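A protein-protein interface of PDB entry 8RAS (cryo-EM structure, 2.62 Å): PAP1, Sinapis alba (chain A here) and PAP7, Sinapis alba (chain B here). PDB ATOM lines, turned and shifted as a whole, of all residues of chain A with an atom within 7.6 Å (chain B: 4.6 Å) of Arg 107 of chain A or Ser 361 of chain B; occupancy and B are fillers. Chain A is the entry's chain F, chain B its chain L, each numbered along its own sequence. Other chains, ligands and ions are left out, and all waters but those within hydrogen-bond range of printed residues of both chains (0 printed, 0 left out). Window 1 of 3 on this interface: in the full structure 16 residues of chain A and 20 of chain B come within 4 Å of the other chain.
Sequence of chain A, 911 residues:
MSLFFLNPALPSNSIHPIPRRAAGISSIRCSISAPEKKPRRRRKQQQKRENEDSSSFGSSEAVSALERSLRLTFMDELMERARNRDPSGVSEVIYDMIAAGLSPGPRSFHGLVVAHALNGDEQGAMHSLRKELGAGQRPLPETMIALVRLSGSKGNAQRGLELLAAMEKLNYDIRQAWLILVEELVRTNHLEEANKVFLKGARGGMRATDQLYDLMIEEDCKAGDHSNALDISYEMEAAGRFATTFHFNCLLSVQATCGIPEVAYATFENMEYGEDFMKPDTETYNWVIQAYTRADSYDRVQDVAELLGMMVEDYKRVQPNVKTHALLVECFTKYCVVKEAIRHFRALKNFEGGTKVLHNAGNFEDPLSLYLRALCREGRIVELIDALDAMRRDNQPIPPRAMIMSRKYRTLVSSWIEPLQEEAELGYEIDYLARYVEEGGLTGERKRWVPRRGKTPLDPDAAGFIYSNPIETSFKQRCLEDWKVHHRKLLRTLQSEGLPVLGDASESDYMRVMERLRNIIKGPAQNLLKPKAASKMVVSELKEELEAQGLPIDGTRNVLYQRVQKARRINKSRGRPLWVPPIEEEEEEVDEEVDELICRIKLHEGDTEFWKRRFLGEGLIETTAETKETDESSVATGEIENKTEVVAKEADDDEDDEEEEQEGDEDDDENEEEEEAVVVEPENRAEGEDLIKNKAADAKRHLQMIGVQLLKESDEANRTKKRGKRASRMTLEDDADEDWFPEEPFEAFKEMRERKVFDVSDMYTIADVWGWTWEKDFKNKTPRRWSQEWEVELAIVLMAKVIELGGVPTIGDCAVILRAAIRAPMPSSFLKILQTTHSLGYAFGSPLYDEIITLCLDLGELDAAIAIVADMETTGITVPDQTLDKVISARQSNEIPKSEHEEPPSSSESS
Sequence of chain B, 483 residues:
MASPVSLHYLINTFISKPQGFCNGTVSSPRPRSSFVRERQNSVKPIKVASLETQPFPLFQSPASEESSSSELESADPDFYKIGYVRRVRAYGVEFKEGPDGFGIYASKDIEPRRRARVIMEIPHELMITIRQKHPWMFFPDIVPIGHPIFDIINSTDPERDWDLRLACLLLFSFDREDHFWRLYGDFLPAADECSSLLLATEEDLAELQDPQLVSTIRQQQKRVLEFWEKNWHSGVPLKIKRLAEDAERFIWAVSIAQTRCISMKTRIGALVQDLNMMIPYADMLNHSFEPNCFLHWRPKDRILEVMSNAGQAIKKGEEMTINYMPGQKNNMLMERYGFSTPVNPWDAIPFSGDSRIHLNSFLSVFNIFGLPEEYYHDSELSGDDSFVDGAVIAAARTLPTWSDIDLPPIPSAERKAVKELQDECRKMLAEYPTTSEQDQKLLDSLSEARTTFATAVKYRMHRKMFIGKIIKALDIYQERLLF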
ATOM      1  N   MET A  75     -29.237  -7.788  25.321  1.00  0.00           N
ATOM      2  CA  MET A  75     -28.322  -6.803  24.761  1.00  0.00           C
ATOM      3  C   MET A  75     -29.070  -5.580  24.259  1.00  0.00           C
ATOM      4  O   MET A  75     -28.608  -4.450  24.438  1.00  0.00           O
ATOM      5  CB  MET A  75     -27.508  -7.428  23.627  1.00  0.00           C
ATOM      6  CG  MET A  75     -26.354  -6.570  23.142  1.00  0.00           C
ATOM      7  SD  MET A  75     -25.053  -6.384  24.373  1.00  0.00           S
ATOM      8  CE  MET A  75     -24.572  -8.094  24.597  1.00  0.00           C
ATOM      9  N   LEU A  78     -30.172  -3.601  27.341  1.00  0.00           N
ATOM     10  CA  LEU A  78     -28.994  -3.005  27.968  1.00  0.00           C
ATOM     11  C   LEU A  78     -28.461  -1.826  27.163  1.00  0.00           C
ATOM     12  O   LEU A  78     -28.109  -0.790  27.734  1.00  0.00           O
ATOM     13  CB  LEU A  78     -27.903  -4.062  28.134  1.00  0.00           C
ATOM     14  CG  LEU A  78     -26.620  -3.634  28.846  1.00  0.00           C
ATOM     15  CD1 LEU A  78     -26.148  -4.717  29.802  1.00  0.00           C
ATOM     16  CD2 LEU A  78     -25.528  -3.293  27.845  1.00  0.00           C
ATOM     17  N   MET A  79     -28.364  -1.975  25.840  1.00  0.00           N
ATOM     18  CA  MET A  79     -27.914  -0.868  25.006  1.00  0.00           C
ATOM     19  C   MET A  79     -28.894   0.289  25.063  1.00  0.00           C
ATOM     20  O   MET A  79     -28.479   1.455  25.024  1.00  0.00           O
ATOM     21  CB  MET A  79     -27.720  -1.330  23.563  1.00  0.00           C
ATOM     22  CG  MET A  79     -26.538  -2.261  23.362  1.00  0.00           C
ATOM     23  SD  MET A  79     -24.966  -1.436  23.652  1.00  0.00           S
ATOM     24  CE  MET A  79     -24.006  -2.777  24.341  1.00  0.00           C
ATOM     25  N   ALA A  82     -28.157   2.043  28.292  1.00  0.00           N
ATOM     26  CA  ALA A  82     -26.920   2.796  28.136  1.00  0.00           C
ATOM     27  C   ALA A  82     -27.136   4.057  27.310  1.00  0.00           C
ATOM     28  O   ALA A  82     -26.458   5.066  27.534  1.00  0.00           O
ATOM     29  CB  ALA A  82     -25.845   1.918  27.498  1.00  0.00           C
ATOM     30  N   VAL A  90     -28.112  -0.347  33.453  1.00  0.00           N
ATOM     31  CA  VAL A  90     -27.206  -1.300  32.822  1.00  0.00           C
ATOM     32  C   VAL A  90     -26.711  -2.314  33.845  1.00  0.00           C
ATOM     33  O   VAL A  90     -26.539  -3.499  33.534  1.00  0.00           O
ATOM     34  CB  VAL A  90     -26.040  -0.563  32.141  1.00  0.00           C
ATOM     35  CG1 VAL A  90     -25.169  -1.550  31.398  1.00  0.00           C
ATOM     36  CG2 VAL A  90     -26.569   0.497  31.192  1.00  0.00           C
ATOM     37  N   ILE A  94     -27.104  -6.326  33.711  1.00  0.00           N
ATOM     38  CA  ILE A  94     -25.973  -7.238  33.862  1.00  0.00           C
ATOM     39  C   ILE A  94     -26.269  -8.281  34.933  1.00  0.00           C
ATOM     40  O   ILE A  94     -25.980  -9.473  34.762  1.00  0.00           O
ATOM     41  CB  ILE A  94     -24.688  -6.448  34.170  1.00  0.00           C
ATOM     42  CG1 ILE A  94     -24.113  -5.862  32.881  1.00  0.00           C
ATOM     43  CG2 ILE A  94     -23.655  -7.334  34.848  1.00  0.00           C
ATOM     44  CD1 ILE A  94     -22.850  -5.062  33.086  1.00  0.00           C
ATOM     45  N   PRO A 104     -21.581 -12.300  30.984  1.00  0.00           N
ATOM     46  CA  PRO A 104     -21.449 -10.933  30.464  1.00  0.00           C
ATOM     47  C   PRO A 104     -20.228 -10.765  29.577  1.00  0.00           C
ATOM     48  O   PRO A 104     -19.090 -10.768  30.059  1.00  0.00           O
ATOM     49  CB  PRO A 104     -21.345 -10.078  31.735  1.00  0.00           C
ATOM     50  CG  PRO A 104     -21.770 -10.974  32.861  1.00  0.00           C
ATOM     51  CD  PRO A 104     -21.397 -12.353  32.441  1.00  0.00           C
ATOM     52  N   GLY A 105     -20.456 -10.613  28.275  1.00  0.00           N
ATOM     53  CA  GLY A 105     -19.378 -10.416  27.340  1.00  0.00           C
ATOM     54  C   GLY A 105     -18.903  -8.982  27.315  1.00  0.00           C
ATOM     55  O   GLY A 105     -19.404  -8.106  28.034  1.00  0.00           O
ATOM     56  N   PRO A 106     -17.899  -8.726  26.476  1.00  0.00           N
ATOM     57  CA  PRO A 106     -17.372  -7.358  26.361  1.00  0.00           C
ATOM     58  C   PRO A 106     -18.388  -6.344  25.866  1.00  0.00           C
ATOM     59  O   PRO A 106     -18.223  -5.154  26.142  1.00  0.00           O
ATOM     60  CB  PRO A 106     -16.208  -7.512  25.370  1.00  0.00           C
ATOM     61  CG  PRO A 106     -15.838  -8.953  25.438  1.00  0.00           C
ATOM     62  CD  PRO A 106     -17.118  -9.688  25.682  1.00  0.00           C
ATOM     63  N   ARG A 107     -19.428  -6.768  25.147  1.00  0.00           N
ATOM     64  CA  ARG A 107     -20.382  -5.810  24.595  1.00  0.00           C
ATOM     65  C   ARG A 107     -21.245  -5.183  25.686  1.00  0.00           C
ATOM     66  O   ARG A 107     -21.410  -3.959  25.735  1.00  0.00           O
ATOM     67  CB  ARG A 107     -21.252  -6.489  23.539  1.00  0.00           C
ATOM     68  CG  ARG A 107     -22.032  -5.526  22.663  1.00  0.00           C
ATOM     69  CD  ARG A 107     -21.132  -4.865  21.632  1.00  0.00           C
ATOM     70  NE  ARG A 107     -20.169  -5.799  21.061  1.00  0.00           N
ATOM     71  CZ  ARG A 107     -19.314  -5.493  20.095  1.00  0.00           C
ATOM     72  NH1 ARG A 107     -19.275  -4.281  19.565  1.00  0.00           N
ATOM     73  NH2 ARG A 107     -18.477  -6.425  19.650  1.00  0.00           N
ATOM     74  N   SER A 108     -21.812  -6.008  26.570  1.00  0.00           N
ATOM     75  CA  SER A 108     -22.651  -5.477  27.643  1.00  0.00           C
ATOM     76  C   SER A 108     -21.842  -4.594  28.583  1.00  0.00           C
ATOM     77  O   SER A 108     -22.296  -3.520  29.002  1.00  0.00           O
ATOM     78  CB  SER A 108     -23.306  -6.614  28.419  1.00  0.00           C
ATOM     79  OG  SER A 108     -24.297  -7.261  27.644  1.00  0.00           O
ATOM     80  N   PHE A 109     -20.639  -5.039  28.932  1.00  0.00           N
ATOM     81  CA  PHE A 109     -19.772  -4.228  29.772  1.00  0.00           C
ATOM     82  C   PHE A 109     -19.352  -2.941  29.076  1.00  0.00           C
ATOM     83  O   PHE A 109     -19.191  -1.909  29.734  1.00  0.00           O
ATOM     84  CB  PHE A 109     -18.547  -5.027  30.176  1.00  0.00           C
ATOM     85  CG  PHE A 109     -18.759  -5.914  31.365  1.00  0.00           C
ATOM     86  CD1 PHE A 109     -18.442  -7.261  31.307  1.00  0.00           C
ATOM     87  CD2 PHE A 109     -19.281  -5.404  32.538  1.00  0.00           C
ATOM     88  CE1 PHE A 109     -18.630  -8.075  32.403  1.00  0.00           C
ATOM     89  CE2 PHE A 109     -19.483  -6.219  33.635  1.00  0.00           C
ATOM     90  CZ  PHE A 109     -19.157  -7.557  33.564  1.00  0.00           C
ATOM     91  N   HIS A 110     -19.151  -2.983  27.759  1.00  0.00           N
ATOM     92  CA  HIS A 110     -18.846  -1.764  27.023  1.00  0.00           C
ATOM     93  C   HIS A 110     -20.019  -0.797  27.076  1.00  0.00           C
ATOM     94  O   HIS A 110     -19.829   0.419  27.187  1.00  0.00           O
ATOM     95  CB  HIS A 110     -18.487  -2.092  25.578  1.00  0.00           C
ATOM     96  CG  HIS A 110     -18.689  -0.950  24.634  1.00  0.00           C
ATOM     97  ND1 HIS A 110     -17.788   0.085  24.519  1.00  0.00           N
ATOM     98  CD2 HIS A 110     -19.690  -0.677  23.762  1.00  0.00           C
ATOM     99  CE1 HIS A 110     -18.222   0.948  23.619  1.00  0.00           C
ATOM    100  NE2 HIS A 110     -19.373   0.509  23.143  1.00  0.00           N
ATOM    101  N   GLY A 111     -21.239  -1.323  26.981  1.00  0.00           N
ATOM    102  CA  GLY A 111     -22.410  -0.485  27.180  1.00  0.00           C
ATOM    103  C   GLY A 111     -22.438   0.142  28.561  1.00  0.00           C
ATOM    104  O   GLY A 111     -22.788   1.313  28.714  1.00  0.00           O
ATOM    105  N   LEU A 112     -22.060  -0.630  29.582  1.00  0.00           N
ATOM    106  CA  LEU A 112     -21.972  -0.085  30.937  1.00  0.00           C
ATOM    107  C   LEU A 112     -20.952   1.046  31.016  1.00  0.00           C
ATOM    108  O   LEU A 112     -21.215   2.101  31.612  1.00  0.00           O
ATOM    109  CB  LEU A 112     -21.613  -1.197  31.924  1.00  0.00           C
ATOM    110  CG  LEU A 112     -21.450  -0.794  33.390  1.00  0.00           C
ATOM    111  CD1 LEU A 112     -22.793  -0.473  34.014  1.00  0.00           C
ATOM    112  CD2 LEU A 112     -20.745  -1.891  34.167  1.00  0.00           C
ATOM    113  N   VAL A 113     -19.775   0.839  30.422  1.00  0.00           N
ATOM    114  CA  VAL A 113     -18.730   1.858  30.457  1.00  0.00           C
ATOM    115  C   VAL A 113     -19.189   3.115  29.730  1.00  0.00           C
ATOM    116  O   VAL A 113     -18.958   4.238  30.195  1.00  0.00           O
ATOM    117  CB  VAL A 113     -17.420   1.313  29.858  1.00  0.00           C
ATOM    118  CG1 VAL A 113     -16.364   2.405  29.822  1.00  0.00           C
ATOM    119  CG2 VAL A 113     -16.925   0.119  30.648  1.00  0.00           C
ATOM    120  N   GLU A 132     -14.495  -5.252  34.130  1.00  0.00           N
ATOM    121  CA  GLU A 132     -13.938  -5.883  32.935  1.00  0.00           C
ATOM    122  C   GLU A 132     -12.818  -6.842  33.297  1.00  0.00           C
ATOM    123  O   GLU A 132     -12.892  -8.049  33.039  1.00  0.00           O
ATOM    124  CB  GLU A 132     -13.382  -4.820  31.976  1.00  0.00           C
ATOM    125  CG  GLU A 132     -13.663  -4.997  30.486  1.00  0.00           C
ATOM    126  CD  GLU A 132     -15.125  -4.982  30.158  1.00  0.00           C
ATOM    127  OE1 GLU A 132     -15.919  -4.870  31.102  1.00  0.00           O
ATOM    128  OE2 GLU A 132     -15.479  -5.074  28.963  1.00  0.00           O
ATOM    129  N   GLN A 137     -12.830 -10.703  30.831  1.00  0.00           N
ATOM    130  CA  GLN A 137     -13.120 -10.368  29.446  1.00  0.00           C
ATOM    131  C   GLN A 137     -12.134  -9.329  28.927  1.00  0.00           C
ATOM    132  O   GLN A 137     -11.618  -8.500  29.680  1.00  0.00           O
ATOM    133  CB  GLN A 137     -14.549  -9.844  29.304  1.00  0.00           C
ATOM    134  CG  GLN A 137     -15.520 -10.395  30.336  1.00  0.00           C
ATOM    135  CD  GLN A 137     -16.036 -11.777  29.982  1.00  0.00           C
ATOM    136  OE1 GLN A 137     -15.523 -12.433  29.076  1.00  0.00           O
ATOM    137  NE2 GLN A 137     -17.059 -12.224  30.699  1.00  0.00           N
ATOM    138  N   ARG A 138     -11.877  -9.384  27.623  1.00  0.00           N
ATOM    139  CA  ARG A 138     -10.986  -8.430  26.980  1.00  0.00           C
ATOM    140  C   ARG A 138     -11.774  -7.191  26.583  1.00  0.00           C
ATOM    141  O   ARG A 138     -12.702  -7.297  25.770  1.00  0.00           O
ATOM    142  CB  ARG A 138     -10.335  -9.050  25.755  1.00  0.00           C
ATOM    143  CG  ARG A 138      -9.160  -8.264  25.204  1.00  0.00           C
ATOM    144  CD  ARG A 138      -8.181  -9.182  24.492  1.00  0.00           C
ATOM    145  NE  ARG A 138      -7.138  -8.439  23.794  1.00  0.00           N
ATOM    146  CZ  ARG A 138      -7.304  -7.835  22.626  1.00  0.00           C
ATOM    147  NH1 ARG A 138      -8.464  -7.862  21.991  1.00  0.00           N
ATOM    148  NH2 ARG A 138      -6.278  -7.189  22.079  1.00  0.00           N
ATOM    149  N   LEU A 140     -13.173  -3.955  24.733  1.00  0.00           N
ATOM    150  CA  LEU A 140     -13.193  -3.582  23.331  1.00  0.00           C
ATOM    151  C   LEU A 140     -12.387  -2.306  23.105  1.00  0.00           C
ATOM    152  O   LEU A 140     -12.171  -1.523  24.034  1.00  0.00           O
ATOM    153  CB  LEU A 140     -14.631  -3.382  22.860  1.00  0.00           C
ATOM    154  CG  LEU A 140     -15.489  -4.640  22.729  1.00  0.00           C
ATOM    155  CD1 LEU A 140     -16.867  -4.281  22.204  1.00  0.00           C
ATOM    156  CD2 LEU A 140     -14.813  -5.654  21.824  1.00  0.00           C
ATOM    157  N   PRO A 141     -11.917  -2.080  21.875  1.00  0.00           N
ATOM    158  CA  PRO A 141     -11.258  -0.798  21.575  1.00  0.00           C
ATOM    159  C   PRO A 141     -12.153   0.403  21.811  1.00  0.00           C
ATOM    160  O   PRO A 141     -11.658   1.463  22.215  1.00  0.00           O
ATOM    161  CB  PRO A 141     -10.879  -0.936  20.094  1.00  0.00           C
ATOM    162  CG  PRO A 141     -10.831  -2.399  19.844  1.00  0.00           C
ATOM    163  CD  PRO A 141     -11.868  -3.009  20.734  1.00  0.00           C
ATOM    164  N   GLU A 142     -13.460   0.271  21.570  1.00  0.00           N
ATOM    165  CA  GLU A 142     -14.373   1.383  21.809  1.00  0.00           C
ATOM    166  C   GLU A 142     -14.451   1.743  23.285  1.00  0.00           C
ATOM    167  O   GLU A 142     -14.587   2.923  23.624  1.00  0.00           O
ATOM    168  CB  GLU A 142     -15.762   1.049  21.269  1.00  0.00           C
ATOM    169  CG  GLU A 142     -15.894   1.228  19.771  1.00  0.00           C
ATOM    170  CD  GLU A 142     -15.493  -0.014  19.006  1.00  0.00           C
ATOM    171  OE1 GLU A 142     -15.545  -1.115  19.592  1.00  0.00           O
ATOM    172  OE2 GLU A 142     -15.118   0.113  17.820  1.00  0.00           O
ATOM    173  N   THR A 143     -14.371   0.751  24.174  1.00  0.00           N
ATOM    174  CA  THR A 143     -14.365   1.036  25.605  1.00  0.00           C
ATOM    175  C   THR A 143     -13.168   1.898  25.987  1.00  0.00           C
ATOM    176  O   THR A 143     -13.309   2.910  26.685  1.00  0.00           O
ATOM    177  CB  THR A 143     -14.355  -0.273  26.394  1.00  0.00           C
ATOM    178  OG1 THR A 143     -15.460  -1.088  25.986  1.00  0.00           O
ATOM    179  CG2 THR A 143     -14.450  -0.002  27.883  1.00  0.00           C
ATOM    180  N   HIS B 358     -23.435   0.536  12.122  1.00  0.00           N
ATOM    181  CA  HIS B 358     -22.492   1.248  12.974  1.00  0.00           C
ATOM    182  C   HIS B 358     -21.073   0.989  12.486  1.00  0.00           C
ATOM    183  O   HIS B 358     -20.628  -0.164  12.435  1.00  0.00           O
ATOM    184  CB  HIS B 358     -22.648   0.820  14.431  1.00  0.00           C
ATOM    185  CG  HIS B 358     -22.054   1.785  15.409  1.00  0.00           C
ATOM    186  ND1 HIS B 358     -21.332   1.380  16.510  1.00  0.00           N
ATOM    187  CD2 HIS B 358     -22.075   3.138  15.450  1.00  0.00           C
ATOM    188  CE1 HIS B 358     -20.934   2.441  17.188  1.00  0.00           C
ATOM    189  NE2 HIS B 358     -21.371   3.521  16.566  1.00  0.00           N
ATOM    190  N   LEU B 359     -20.365   2.061  12.127  1.00  0.00           N
ATOM    191  CA  LEU B 359     -19.009   1.920  11.609  1.00  0.00           C
ATOM    192  C   LEU B 359     -18.057   1.378  12.669  1.00  0.00           C
ATOM    193  O   LEU B 359     -17.232   0.505  12.378  1.00  0.00           O
ATOM    194  CB  LEU B 359     -18.509   3.261  11.078  1.00  0.00           C
ATOM    195  CG  LEU B 359     -17.044   3.312  10.641  1.00  0.00           C
ATOM    196  CD1 LEU B 359     -16.786   2.316   9.522  1.00  0.00           C
ATOM    197  CD2 LEU B 359     -16.660   4.717  10.213  1.00  0.00           C
ATOM    198  N   ASN B 360     -18.153   1.888  13.899  1.00  0.00           N
ATOM    199  CA  ASN B 360     -17.215   1.482  14.942  1.00  0.00           C
ATOM    200  C   ASN B 360     -17.342  -0.002  15.260  1.00  0.00           C
ATOM    201  O   ASN B 360     -16.332  -0.704  15.390  1.00  0.00           O
ATOM    202  CB  ASN B 360     -17.436   2.321  16.200  1.00  0.00           C
ATOM    203  CG  ASN B 360     -17.196   3.798  15.964  1.00  0.00           C
ATOM    204  OD1 ASN B 360     -18.107   4.614  16.099  1.00  0.00           O
ATOM    205  ND2 ASN B 360     -15.966   4.149  15.610  1.00  0.00           N
ATOM    206  N   SER B 361     -18.575  -0.497  15.390  1.00  0.00           N
ATOM    207  CA  SER B 361     -18.773  -1.916  15.667  1.00  0.00           C
ATOM    208  C   SER B 361     -18.288  -2.777  14.508  1.00  0.00           C
ATOM    209  O   SER B 361     -17.683  -3.834  14.723  1.00  0.00           O
ATOM    210  CB  SER B 361     -20.247  -2.191  15.964  1.00  0.00           C
ATOM    211  OG  SER B 361     -20.610  -1.694  17.241  1.00  0.00           O
ATOM    212  N   PHE B 362     -18.548  -2.342  13.273  1.00  0.00           N
ATOM    213  CA  PHE B 362     -18.082  -3.087  12.107  1.00  0.00           C
ATOM    214  C   PHE B 362     -16.561  -3.174  12.082  1.00  0.00           C
ATOM    215  O   PHE B 362     -15.997  -4.232  11.781  1.00  0.00           O
ATOM    216  CB  PHE B 362     -18.606  -2.433  10.829  1.00  0.00           C
ATOM    217  CG  PHE B 362     -18.466  -3.289   9.602  1.00  0.00           C
ATOM    218  CD1 PHE B 362     -17.291  -3.289   8.869  1.00  0.00           C
ATOM    219  CD2 PHE B 362     -19.512  -4.087   9.176  1.00  0.00           C
ATOM    220  CE1 PHE B 362     -17.162  -4.072   7.741  1.00  0.00           C
ATOM    221  CE2 PHE B 362     -19.389  -4.870   8.047  1.00  0.00           C
ATOM    222  CZ  PHE B 362     -18.213  -4.863   7.330  1.00  0.00           C
ATOM    223  N   LEU B 363     -15.881  -2.068  12.390  1.00  0.00           N
ATOM    224  CA  LEU B 363     -14.423  -2.086  12.425  1.00  0.00           C
ATOM    225  C   LEU B 363     -13.902  -2.962  13.557  1.00  0.00           C
ATOM    226  O   LEU B 363     -12.942  -3.718  13.372  1.00  0.00           O
ATOM    227  CB  LEU B 363     -13.883  -0.663  12.560  1.00  0.00           C
ATOM    228  CG  LEU B 363     -14.205   0.318  11.434  1.00  0.00           C
ATOM    229  CD1 LEU B 363     -13.578   1.672  11.717  1.00  0.00           C
ATOM    230  CD2 LEU B 363     -13.739  -0.223  10.095  1.00  0.00           C
ATOM    231  N   SER B 364     -14.519  -2.874  14.739  1.00  0.00           N
ATOM    232  CA  SER B 364     -14.014  -3.612  15.892  1.00  0.00           C
ATOM    233  C   SER B 364     -14.239  -5.111  15.755  1.00  0.00           C
ATOM    234  O   SER B 364     -13.404  -5.903  16.206  1.00  0.00           O
ATOM    235  CB  SER B 364     -14.666  -3.097  17.173  1.00  0.00           C
ATOM    236  OG  SER B 364     -16.039  -3.442  17.220  1.00  0.00           O
ATOM    237  N   VAL B 365     -15.357  -5.522  15.153  1.00  0.00           N
ATOM    238  CA  VAL B 365     -15.632  -6.947  14.992  1.00  0.00           C
ATOM    239  C   VAL B 365     -14.598  -7.593  14.081  1.00  0.00           C
ATOM    240  O   VAL B 365     -14.077  -8.676  14.375  1.00  0.00           O
ATOM    241  CB  VAL B 365     -17.065  -7.158  14.469  1.00  0.00           C
ATOM    242  CG1 VAL B 365     -17.222  -8.550  13.892  1.00  0.00           C
ATOM    243  CG2 VAL B 365     -18.071  -6.928  15.582  1.00  0.00           C
ATOM    244  N   PRO B 409     -24.779   1.113  19.307  1.00  0.00           N
ATOM    245  CA  PRO B 409     -25.945   0.741  18.499  1.00  0.00           C
ATOM    246  C   PRO B 409     -26.808  -0.307  19.183  1.00  0.00           C
ATOM    247  O   PRO B 409     -26.288  -1.286  19.726  1.00  0.00           O
ATOM    248  CB  PRO B 409     -25.308   0.196  17.218  1.00  0.00           C
ATOM    249  CG  PRO B 409     -24.014  -0.409  17.689  1.00  0.00           C
ATOM    250  CD  PRO B 409     -23.585   0.333  18.942  1.00  0.00           C
ATOM    251  N   TYR B 477     -21.154 -10.037  11.032  1.00  0.00           N
ATOM    252  CA  TYR B 477     -21.153  -8.876  11.915  1.00  0.00           C
ATOM    253  C   TYR B 477     -22.414  -8.829  12.765  1.00  0.00           C
ATOM    254  O   TYR B 477     -22.350  -8.534  13.964  1.00  0.00           O
ATOM    255  CB  TYR B 477     -21.004  -7.599  11.091  1.00  0.00           C
ATOM    256  CG  TYR B 477     -21.612  -6.367  11.721  1.00  0.00           C
ATOM    257  CD1 TYR B 477     -20.991  -5.728  12.783  1.00  0.00           C
ATOM    258  CD2 TYR B 477     -22.802  -5.835  11.243  1.00  0.00           C
ATOM    259  CE1 TYR B 477     -21.541  -4.599  13.357  1.00  0.00           C
ATOM    260  CE2 TYR B 477     -23.359  -4.708  11.810  1.00  0.00           C
ATOM    261  CZ  TYR B 477     -22.724  -4.094  12.867  1.00  0.00           C
ATOM    262  OH  TYR B 477     -23.275  -2.970  13.436  1.00  0.00           O
ATOM    263  N   ARG B 480     -21.903 -11.539  15.488  1.00  0.00           N
ATOM    264  CA  ARG B 480     -20.986 -11.221  16.573  1.00  0.00           C
ATOM    265  C   ARG B 480     -21.331  -9.916  17.283  1.00  0.00           C
ATOM    266  O   ARG B 480     -20.498  -9.389  18.029  1.00  0.00           O
ATOM    267  CB  ARG B 480     -19.546 -11.164  16.055  1.00  0.00           C
ATOM    268  CG  ARG B 480     -18.527 -11.715  17.039  1.00  0.00           C
ATOM    269  CD  ARG B 480     -17.291 -12.254  16.339  1.00  0.00           C
ATOM    270  NE  ARG B 480     -17.145 -11.725  14.989  1.00  0.00           N
ATOM    271  CZ  ARG B 480     -16.579 -12.380  13.985  1.00  0.00           C
ATOM    272  NH1 ARG B 480     -16.100 -13.603  14.140  1.00  0.00           N
ATOM    273  NH2 ARG B 480     -16.484 -11.789  12.798  1.00  0.00           N
ATOM    274  N   LEU B 481     -22.533  -9.383  17.072  1.00  0.00           N
ATOM    275  CA  LEU B 481     -22.940  -8.159  17.749  1.00  0.00           C
ATOM    276  C   LEU B 481     -23.361  -8.392  19.193  1.00  0.00           C
ATOM    277  O   LEU B 481     -23.553  -7.419  19.930  1.00  0.00           O
ATOM    278  CB  LEU B 481     -24.085  -7.492  16.983  1.00  0.00           C
ATOM    279  CG  LEU B 481     -24.188  -5.971  17.105  1.00  0.00           C
ATOM    280  CD1 LEU B 481     -22.955  -5.303  16.528  1.00  0.00           C
ATOM    281  CD2 LEU B 481     -25.448  -5.461  16.425  1.00  0.00           C
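OG of Ser 364 of chain B sits close to OE1 of Glu 142 of chain A (3.4 Å). The side-chain carboxylate (OE2) of Glu 142 of chain A sits close to the backbone carbonyl oxygen (O) of Asn 360 of chain B, at 2.8 Å.
The side-chain amide oxygen (OD1) of Asn 360 of chain B sits at hydrogen-bond distance from a ring nitrogen (NE2) of His 358 of chain B (3.5 Å). ND1 of His 358 of chain B is in hydrogen-bond range of OG of Ser 361 of chain B. The side-chain hydroxyl (OG) of Ser 364 of chain B lies within hydrogen-bond range of the backbone carbonyl oxygen (O) of Asn 360 of chain B, 3.3 Å away. The backbone carbonyl oxygen of Ser 361 of chain B lies within hydrogen-bond range of the side-chain hydroxyl of Ser 364 of chain B (3.0 Å).
Among the printed residues, pairs that only touch across the chains: Met 79 of chain A with Pro 409 of chain B (3.8 Å), Arg 107 of chain A with Ser 361 of chain B (3.7 Å), Arg 107 of chain A with Arg 480 of chain B (3.9 Å) and Arg 107 of chain A with Leu 481 of chain B (3.7 Å).
Of chain B, only Ser 361, Arg 480 and Leu 481 come within 4 Å of Arg 107 of chain A. Of the printed residues of chain B, Glu 142 of chain A touches Asn 360 (2.8 Å) and Ser 364 (3.2 Å). Of the printed residues of chain A, Asn 360 of chain B touches Glu 142 (2.8 Å). Of chain A, only Arg 107 (3.7 Å) comes within 4 Å of Ser 361 of chain B. Printed residues of chain A within 4 Å of Pro 409 of chain B: Met 79 (3.8 Å). Of the printed residues of chain A, Arg 480 of chain B touches Arg 107 (3.9 Å). Of the printed residues of chain A, Leu 481 of chain B touches Arg 107 (3.7 Å). The nearest residue of chain A that does not touch Ser 361 of chain B is Glu 142 of chain A (4.3 Å). The nearest printed residue of chain A that does not touch Leu 481 of chain B is Met 75 of chain A (4.3 Å).
Of the 12 printed residues of chain B, 6 touch a printed residue of chain A. Along chain B the printed residues that touch a printed residue of chain A span positions 360 to 481. Hydrophobic or aromatic side chains of chain A that line the printed part of chain B: Met 79. Among the printed residues, 6 pairs touch across the chains. Among the printed residues, no Asp or Glu carboxylate lies within 4 Å of a Lys or Arg side-chain nitrogen of the other chain.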
